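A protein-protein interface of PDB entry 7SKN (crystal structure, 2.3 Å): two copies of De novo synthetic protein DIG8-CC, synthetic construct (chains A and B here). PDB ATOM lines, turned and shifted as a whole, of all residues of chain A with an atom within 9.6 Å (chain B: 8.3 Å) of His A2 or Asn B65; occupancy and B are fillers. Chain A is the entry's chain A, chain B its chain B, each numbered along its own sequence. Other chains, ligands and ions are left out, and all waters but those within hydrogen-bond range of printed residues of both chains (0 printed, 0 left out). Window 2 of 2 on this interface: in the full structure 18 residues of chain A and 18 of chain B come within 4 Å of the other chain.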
ATOM      1  N   HIS A   2     -29.601  -4.617  18.151  1.00  0.00           N
ATOM      2  CA  HIS A   2     -29.315  -3.724  19.268  1.00  0.00           C
ATOM      3  C   HIS A   2     -28.293  -2.661  18.874  1.00  0.00           C
ATOM      4  O   HIS A   2     -27.343  -2.941  18.138  1.00  0.00           O
ATOM      5  CB  HIS A   2     -28.809  -4.520  20.475  1.00  0.00           C
ATOM      6  CG  HIS A   2     -28.664  -3.703  21.721  1.00  0.00           C
ATOM      7  ND1 HIS A   2     -27.561  -2.915  21.971  1.00  0.00           N
ATOM      8  CD2 HIS A   2     -29.484  -3.551  22.788  1.00  0.00           C
ATOM      9  CE1 HIS A   2     -27.708  -2.312  23.138  1.00  0.00           C
ATOM     10  NE2 HIS A   2     -28.866  -2.682  23.655  1.00  0.00           N
ATOM     11  N   MET A   3     -28.490  -1.441  19.370  1.00  0.00           N
ATOM     12  CA  MET A   3     -27.584  -0.334  19.086  1.00  0.00           C
ATOM     13  C   MET A   3     -26.391  -0.430  20.030  1.00  0.00           C
ATOM     14  O   MET A   3     -26.526  -0.210  21.237  1.00  0.00           O
ATOM     15  CB  MET A   3     -28.306   1.000  19.243  1.00  0.00           C
ATOM     16  CG  MET A   3     -27.708   2.139  18.431  1.00  0.00           C
ATOM     17  SD  MET A   3     -27.860   1.876  16.653  1.00  0.00           S
ATOM     18  CE  MET A   3     -29.613   1.528  16.506  1.00  0.00           C
ATOM     19  N   ARG A   4     -25.222  -0.755  19.482  1.00  0.00           N
ATOM     20  CA  ARG A   4     -24.035  -0.978  20.299  1.00  0.00           C
ATOM     21  C   ARG A   4     -23.252   0.304  20.554  1.00  0.00           C
ATOM     22  O   ARG A   4     -22.959   0.632  21.707  1.00  0.00           O
ATOM     23  CB  ARG A   4     -23.133  -2.020  19.637  1.00  0.00           C
ATOM     24  CG  ARG A   4     -23.657  -3.433  19.733  1.00  0.00           C
ATOM     25  CD  ARG A   4     -22.577  -4.338  20.275  1.00  0.00           C
ATOM     26  NE  ARG A   4     -21.309  -4.097  19.600  1.00  0.00           N
ATOM     27  CZ  ARG A   4     -20.166  -4.692  19.911  1.00  0.00           C
ATOM     28  NH1 ARG A   4     -20.095  -5.581  20.889  1.00  0.00           N
ATOM     29  NH2 ARG A   4     -19.068  -4.386  19.227  1.00  0.00           N
ATOM     30  N   ILE A   5     -22.895   1.031  19.498  1.00  0.00           N
ATOM     31  CA  ILE A   5     -22.064   2.228  19.606  1.00  0.00           C
ATOM     32  C   ILE A   5     -22.725   3.340  18.808  1.00  0.00           C
ATOM     33  O   ILE A   5     -22.706   3.311  17.573  1.00  0.00           O
ATOM     34  CB  ILE A   5     -20.632   1.990  19.106  1.00  0.00           C
ATOM     35  CG1 ILE A   5     -19.930   0.959  19.983  1.00  0.00           C
ATOM     36  CG2 ILE A   5     -19.860   3.297  19.092  1.00  0.00           C
ATOM     37  CD1 ILE A   5     -19.870   1.358  21.437  1.00  0.00           C
ATOM     38  N   GLU A   6     -23.263   4.341  19.500  1.00  0.00           N
ATOM     39  CA  GLU A   6     -23.930   5.474  18.875  1.00  0.00           C
ATOM     40  C   GLU A   6     -23.111   6.738  19.105  1.00  0.00           C
ATOM     41  O   GLU A   6     -22.753   7.048  20.246  1.00  0.00           O
ATOM     42  CB  GLU A   6     -25.343   5.639  19.439  1.00  0.00           C
ATOM     43  CG  GLU A   6     -26.194   6.679  18.731  1.00  0.00           C
ATOM     44  CD  GLU A   6     -27.650   6.634  19.164  1.00  0.00           C
ATOM     45  OE1 GLU A   6     -28.035   5.682  19.877  1.00  0.00           O
ATOM     46  OE2 GLU A   6     -28.413   7.551  18.788  1.00  0.00           O
ATOM     47  N   ARG A  17     -22.888   6.866  23.078  1.00  0.00           N
ATOM     48  CA  ARG A  17     -23.627   5.934  23.919  1.00  0.00           C
ATOM     49  C   ARG A  17     -23.043   4.537  23.758  1.00  0.00           C
ATOM     50  O   ARG A  17     -22.805   4.086  22.634  1.00  0.00           O
ATOM     51  CB  ARG A  17     -25.118   5.936  23.569  1.00  0.00           C
ATOM     52  CG  ARG A  17     -25.884   4.739  24.117  1.00  0.00           C
ATOM     53  CD  ARG A  17     -27.384   4.992  24.165  1.00  0.00           C
ATOM     54  NE  ARG A  17     -27.741   5.922  25.230  1.00  0.00           N
ATOM     55  CZ  ARG A  17     -27.865   5.586  26.508  1.00  0.00           C
ATOM     56  NH1 ARG A  17     -27.659   4.344  26.918  1.00  0.00           N
ATOM     57  NH2 ARG A  17     -28.197   6.519  27.396  1.00  0.00           N
ATOM     58  N   ASN A  18     -22.809   3.862  24.884  1.00  0.00           N
ATOM     59  CA  ASN A  18     -22.266   2.507  24.900  1.00  0.00           C
ATOM     60  C   ASN A  18     -23.415   1.526  25.106  1.00  0.00           C
ATOM     61  O   ASN A  18     -24.003   1.465  26.190  1.00  0.00           O
ATOM     62  CB  ASN A  18     -21.215   2.360  26.001  1.00  0.00           C
ATOM     63  CG  ASN A  18     -20.537   0.998  25.994  1.00  0.00           C
ATOM     64  OD1 ASN A  18     -20.933   0.090  25.262  1.00  0.00           O
ATOM     65  ND2 ASN A  18     -19.509   0.848  26.822  1.00  0.00           N
ATOM     66  N   GLY A  19     -23.726   0.755  24.067  1.00  0.00           N
ATOM     67  CA  GLY A  19     -24.721  -0.294  24.138  1.00  0.00           C
ATOM     68  C   GLY A  19     -24.168  -1.680  24.382  1.00  0.00           C
ATOM     69  O   GLY A  19     -24.935  -2.650  24.339  1.00  0.00           O
ATOM     70  N   THR A  20     -22.869  -1.811  24.634  1.00  0.00           N
ATOM     71  CA  THR A  20     -22.245  -3.101  24.875  1.00  0.00           C
ATOM     72  C   THR A  20     -22.382  -3.488  26.346  1.00  0.00           C
ATOM     73  O   THR A  20     -22.962  -2.761  27.157  1.00  0.00           O
ATOM     74  CB  THR A  20     -20.775  -3.068  24.461  1.00  0.00           C
ATOM     75  OG1 THR A  20     -20.045  -2.230  25.366  1.00  0.00           O
ATOM     76  CG2 THR A  20     -20.635  -2.515  23.052  1.00  0.00           C
ATOM     77  N   ASP A  21     -21.837  -4.652  26.697  1.00  0.00           N
ATOM     78  CA  ASP A  21     -21.853  -5.152  28.065  1.00  0.00           C
ATOM     79  C   ASP A  21     -20.547  -4.882  28.803  1.00  0.00           C
ATOM     80  O   ASP A  21     -20.386  -5.334  29.941  1.00  0.00           O
ATOM     81  CB  ASP A  21     -22.157  -6.652  28.077  1.00  0.00           C
ATOM     82  CG  ASP A  21     -23.542  -6.970  27.552  1.00  0.00           C
ATOM     83  OD1 ASP A  21     -24.465  -6.159  27.778  1.00  0.00           O
ATOM     84  OD2 ASP A  21     -23.711  -8.032  26.915  1.00  0.00           O
ATOM     85  N   PRO A  41     -21.019   0.892  30.272  1.00  0.00           N
ATOM     86  CA  PRO A  41     -22.171   0.365  29.529  1.00  0.00           C
ATOM     87  C   PRO A  41     -23.483   0.948  30.032  1.00  0.00           C
ATOM     88  O   PRO A  41     -23.688   1.127  31.235  1.00  0.00           O
ATOM     89  CB  PRO A  41     -22.093  -1.147  29.779  1.00  0.00           C
ATOM     90  CG  PRO A  41     -21.248  -1.294  31.008  1.00  0.00           C
ATOM     91  CD  PRO A  41     -20.252  -0.181  30.927  1.00  0.00           C
ATOM     92  N   GLY A  42     -24.382   1.230  29.092  1.00  0.00           N
ATOM     93  CA  GLY A  42     -25.668   1.816  29.415  1.00  0.00           C
ATOM     94  C   GLY A  42     -25.640   3.297  29.700  1.00  0.00           C
ATOM     95  O   GLY A  42     -26.665   3.853  30.112  1.00  0.00           O
ATOM     96  N   THR A  43     -24.506   3.956  29.490  1.00  0.00           N
ATOM     97  CA  THR A  43     -24.343   5.370  29.780  1.00  0.00           C
ATOM     98  C   THR A  43     -24.067   6.131  28.492  1.00  0.00           C
ATOM     99  O   THR A  43     -23.816   5.550  27.432  1.00  0.00           O
ATOM    100  CB  THR A  43     -23.204   5.609  30.778  1.00  0.00           C
ATOM    101  OG1 THR A  43     -21.950   5.295  30.157  1.00  0.00           O
ATOM    102  CG2 THR A  43     -23.381   4.738  32.009  1.00  0.00           C
ATOM    103  N   ARG B   4     -12.906  -1.913  12.864  1.00  0.00           N
ATOM    104  CA  ARG B   4     -14.027  -2.688  12.341  1.00  0.00           C
ATOM    105  C   ARG B   4     -14.896  -1.849  11.412  1.00  0.00           C
ATOM    106  O   ARG B   4     -15.275  -2.300  10.327  1.00  0.00           O
ATOM    107  CB  ARG B   4     -14.859  -3.259  13.489  1.00  0.00           C
ATOM    108  CG  ARG B   4     -14.559  -4.715  13.803  1.00  0.00           C
ATOM    109  CD  ARG B   4     -15.319  -5.189  15.032  1.00  0.00           C
ATOM    110  NE  ARG B   4     -16.766  -5.116  14.858  1.00  0.00           N
ATOM    111  CZ  ARG B   4     -17.532  -6.139  14.502  1.00  0.00           C
ATOM    112  NH1 ARG B   4     -17.018  -7.333  14.257  1.00  0.00           N
ATOM    113  NH2 ARG B   4     -18.845  -5.959  14.396  1.00  0.00           N
ATOM    114  N   ARG B  22     -17.724 -10.183   7.308  1.00  0.00           N
ATOM    115  CA  ARG B  22     -18.995 -10.450   6.656  1.00  0.00           C
ATOM    116  C   ARG B  22     -19.588  -9.151   6.132  1.00  0.00           C
ATOM    117  O   ARG B  22     -19.278  -8.071   6.645  1.00  0.00           O
ATOM    118  CB  ARG B  22     -19.982 -11.123   7.622  1.00  0.00           C
ATOM    119  CG  ARG B  22     -19.589 -12.542   8.011  1.00  0.00           C
ATOM    120  CD  ARG B  22     -20.631 -13.182   8.912  1.00  0.00           C
ATOM    121  NE  ARG B  22     -20.847 -12.408  10.128  1.00  0.00           N
ATOM    122  CZ  ARG B  22     -20.100 -12.504  11.219  1.00  0.00           C
ATOM    123  NH1 ARG B  22     -19.070 -13.332  11.281  1.00  0.00           N
ATOM    124  NH2 ARG B  22     -20.393 -11.748  12.274  1.00  0.00           N
ATOM    125  N   VAL B  61     -25.121   1.525  10.353  1.00  0.00           N
ATOM    126  CA  VAL B  61     -24.435   0.335   9.866  1.00  0.00           C
ATOM    127  C   VAL B  61     -24.887  -0.851  10.703  1.00  0.00           C
ATOM    128  O   VAL B  61     -24.881  -0.782  11.938  1.00  0.00           O
ATOM    129  CB  VAL B  61     -22.905   0.495   9.928  1.00  0.00           C
ATOM    130  CG1 VAL B  61     -22.220  -0.716   9.313  1.00  0.00           C
ATOM    131  CG2 VAL B  61     -22.476   1.773   9.226  1.00  0.00           C
ATOM    132  N   GLU B  62     -25.290  -1.929  10.036  1.00  0.00           N
ATOM    133  CA  GLU B  62     -25.700  -3.156  10.707  1.00  0.00           C
ATOM    134  C   GLU B  62     -24.803  -4.294  10.246  1.00  0.00           C
ATOM    135  O   GLU B  62     -24.778  -4.623   9.055  1.00  0.00           O
ATOM    136  CB  GLU B  62     -27.165  -3.487  10.422  1.00  0.00           C
ATOM    137  CG  GLU B  62     -27.678  -4.661  11.240  1.00  0.00           C
ATOM    138  CD  GLU B  62     -28.972  -5.233  10.703  1.00  0.00           C
ATOM    139  OE1 GLU B  62     -29.095  -5.371   9.467  1.00  0.00           O
ATOM    140  OE2 GLU B  62     -29.866  -5.547  11.516  1.00  0.00           O
ATOM    141  N   CYS B  63     -24.080  -4.893  11.185  1.00  0.00           N
ATOM    142  CA  CYS B  63     -23.234  -6.053  10.910  1.00  0.00           C
ATOM    143  C   CYS B  63     -23.791  -7.219  11.720  1.00  0.00           C
ATOM    144  O   CYS B  63     -23.524  -7.341  12.920  1.00  0.00           O
ATOM    145  CB  CYS B  63     -21.771  -5.768  11.238  1.00  0.00           C
ATOM    146  SG  CYS B  63     -20.993  -4.475  10.217  1.00  0.00           S
ATOM    147  N   GLY B  64     -24.570  -8.065  11.060  1.00  0.00           N
ATOM    148  CA  GLY B  64     -25.224  -9.157  11.758  1.00  0.00           C
ATOM    149  C   GLY B  64     -26.380  -8.627  12.567  1.00  0.00           C
ATOM    150  O   GLY B  64     -27.269  -7.955  12.039  1.00  0.00           O
ATOM    151  N   ASN B  65     -26.368  -8.915  13.865  1.00  0.00           N
ATOM    152  CA  ASN B  65     -27.385  -8.422  14.781  1.00  0.00           C
ATOM    153  C   ASN B  65     -26.948  -7.151  15.497  1.00  0.00           C
ATOM    154  O   ASN B  65     -27.654  -6.681  16.394  1.00  0.00           O
ATOM    155  CB  ASN B  65     -27.743  -9.507  15.798  1.00  0.00           C
ATOM    156  CG  ASN B  65     -28.245 -10.778  15.138  1.00  0.00           C
ATOM    157  OD1 ASN B  65     -28.911 -10.732  14.102  1.00  0.00           O
ATOM    158  ND2 ASN B  65     -27.925 -11.921  15.733  1.00  0.00           N
ATOM    159  N   GLU B  66     -25.807  -6.584  15.118  1.00  0.00           N
ATOM    160  CA  GLU B  66     -25.238  -5.420  15.782  1.00  0.00           C
ATOM    161  C   GLU B  66     -25.415  -4.192  14.897  1.00  0.00           C
ATOM    162  O   GLU B  66     -25.099  -4.230  13.702  1.00  0.00           O
ATOM    163  CB  GLU B  66     -23.757  -5.650  16.094  1.00  0.00           C
ATOM    164  CG  GLU B  66     -23.409  -7.104  16.420  1.00  0.00           C
ATOM    165  CD  GLU B  66     -23.340  -7.392  17.913  1.00  0.00           C
ATOM    166  OE1 GLU B  66     -22.324  -7.036  18.546  1.00  0.00           O
ATOM    167  OE2 GLU B  66     -24.299  -7.981  18.454  1.00  0.00           O
ATOM    168  N   LYS B  67     -25.934  -3.112  15.483  1.00  0.00           N
ATOM    169  CA  LYS B  67     -26.076  -1.825  14.818  1.00  0.00           C
ATOM    170  C   LYS B  67     -25.263  -0.774  15.568  1.00  0.00           C
ATOM    171  O   LYS B  67     -25.100  -0.853  16.790  1.00  0.00           O
ATOM    172  CB  LYS B  67     -27.545  -1.387  14.736  1.00  0.00           C
ATOM    173  CG  LYS B  67     -28.466  -2.335  13.965  1.00  0.00           C
ATOM    174  CD  LYS B  67     -29.874  -1.751  13.852  1.00  0.00           C
ATOM    175  CE  LYS B  67     -30.783  -2.607  12.976  1.00  0.00           C
ATOM    176  NZ  LYS B  67     -32.160  -2.036  12.846  1.00  0.00           N
ATOM    177  N   TYR B  68     -24.723   0.197  14.825  1.00  0.00           N
ATOM    178  CA  TYR B  68     -23.894   1.238  15.429  1.00  0.00           C
ATOM    179  C   TYR B  68     -24.465   2.639  15.249  1.00  0.00           C
ATOM    180  O   TYR B  68     -24.815   3.282  16.241  1.00  0.00           O
ATOM    181  CB  TYR B  68     -22.477   1.118  14.850  1.00  0.00           C
ATOM    182  CG  TYR B  68     -21.871  -0.234  15.151  1.00  0.00           C
ATOM    183  CD1 TYR B  68     -21.167  -0.443  16.327  1.00  0.00           C
ATOM    184  CD2 TYR B  68     -22.034  -1.308  14.284  1.00  0.00           C
ATOM    185  CE1 TYR B  68     -20.626  -1.672  16.626  1.00  0.00           C
ATOM    186  CE2 TYR B  68     -21.490  -2.547  14.576  1.00  0.00           C
ATOM    187  CZ  TYR B  68     -20.787  -2.718  15.750  1.00  0.00           C
ATOM    188  OH  TYR B  68     -20.240  -3.940  16.060  1.00  0.00           O
ATOM    189  N   ARG B  69     -24.618   3.113  14.014  1.00  0.00           N
ATOM    190  CA  ARG B  69     -25.205   4.416  13.703  1.00  0.00           C
ATOM    191  C   ARG B  69     -24.292   5.587  14.067  1.00  0.00           C
ATOM    192  O   ARG B  69     -23.814   5.692  15.201  1.00  0.00           O
ATOM    193  CB  ARG B  69     -26.569   4.593  14.382  1.00  0.00           C
ATOM    194  CG  ARG B  69     -27.189   5.962  14.135  1.00  0.00           C
ATOM    195  CD  ARG B  69     -28.702   5.926  14.190  1.00  0.00           C
ATOM    196  NE  ARG B  69     -29.189   5.830  15.557  1.00  0.00           N
ATOM    197  CZ  ARG B  69     -30.337   5.264  15.901  1.00  0.00           C
ATOM    198  NH1 ARG B  69     -31.116   4.683  15.003  1.00  0.00           N
ATOM    199  NH2 ARG B  69     -30.709   5.278  17.177  1.00  0.00           N
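The backbone NH of Gly A19 is in hydrogen-bond range of the backbone carbonyl oxygen of Arg A4. The backbone carbonyl oxygen (O) of Glu A6 sits at hydrogen-bond distance from the backbone NH (N) of Arg A17, 2.8 Å away. OH of Tyr B68 is in hydrogen-bond range of NH2 of Arg B4 (3.0 Å). N of Tyr B68 lies within hydrogen-bond range of O of Val B61 (3.1 Å).
N of His A2 sits at hydrogen-bond distance from O of Asn B65, at 3.3 Å. O of His A2 lies within hydrogen-bond range of N of Lys B67 (3.0 Å). NE of Arg A4 lies within salt-bridge range of OE1 of Glu B66 (3.3 Å). The backbone NH (N) of Arg A4 is in hydrogen-bond range of the backbone carbonyl oxygen (O) of Lys B67 (2.7 Å). The guanidinium group of Arg A4 is in hydrogen-bond range of the side-chain hydroxyl of Tyr B68. O of Ile A5 sits close to O of Tyr B68, at 2.5 Å. OE2 of Glu A6 is in salt-bridge range of NH2 of Arg B69 (3.6 Å). O of Tyr B68 lies close to SD of Met A3, 3.4 Å away.
Among the printed residues, pairs that only touch across the chains: His A2 with Glu B66 (3.97 Å), Met A3 with Lys B67 (3.4 Å), Met A3 with Arg B69 (3.8 Å), Ile A5 with Lys B67 (3.97 Å), Ile A5 with Arg B69 (3.5 Å) and Glu A6 with Tyr B68 (3.5 Å).
Position printed for both chains: 4. Of the 14 pairs that touch across the chains among the printed residues, none has its exchanged pair printed and touching as well.
His A2 touches just these residues of chain B: Asn B65, Glu B66 and Lys B67. Of the printed residues of chain B, Met A3 touches Lys B67 (3.4 Å), Tyr B68 (3.4 Å) and Arg B69 (3.8 Å). Of the printed residues of chain B, Ile A5 touches Lys B67 (3.97 Å), Tyr B68 (2.5 Å) and Arg B69 (3.5 Å). Of the printed residues of chain B, Glu A6 touches Tyr B68 and Arg B69. Asp A21 touches none of the printed residues of chain B. No residue of chain A comes within 4 Å of Gly B64. Printed residues of chain A within 4 Å of Lys B67: His A2, Met A3, Arg A4 and Ile A5. Printed residues of chain A within 4 Å of Arg B69: Met A3, Ile A5 and Glu A6. The nearest residue of chain B that does not touch His A2 is Tyr B68 (5.3 Å). The nearest residue of chain A that does not touch Asn B65 is Met A3 (6.1 Å). The nearest printed residue of chain B that does not touch Ile A5 is Val B61 (7.3 Å).
Hydrophobic or aromatic side chains of chain B that line the printed part of chain A: Tyr B68. Among the printed residues, Asp or Glu carboxylates within 4 Å of a Lys or Arg side-chain nitrogen of the other chain: Arg A4 with Glu B66 and Glu A6 with Arg B69.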
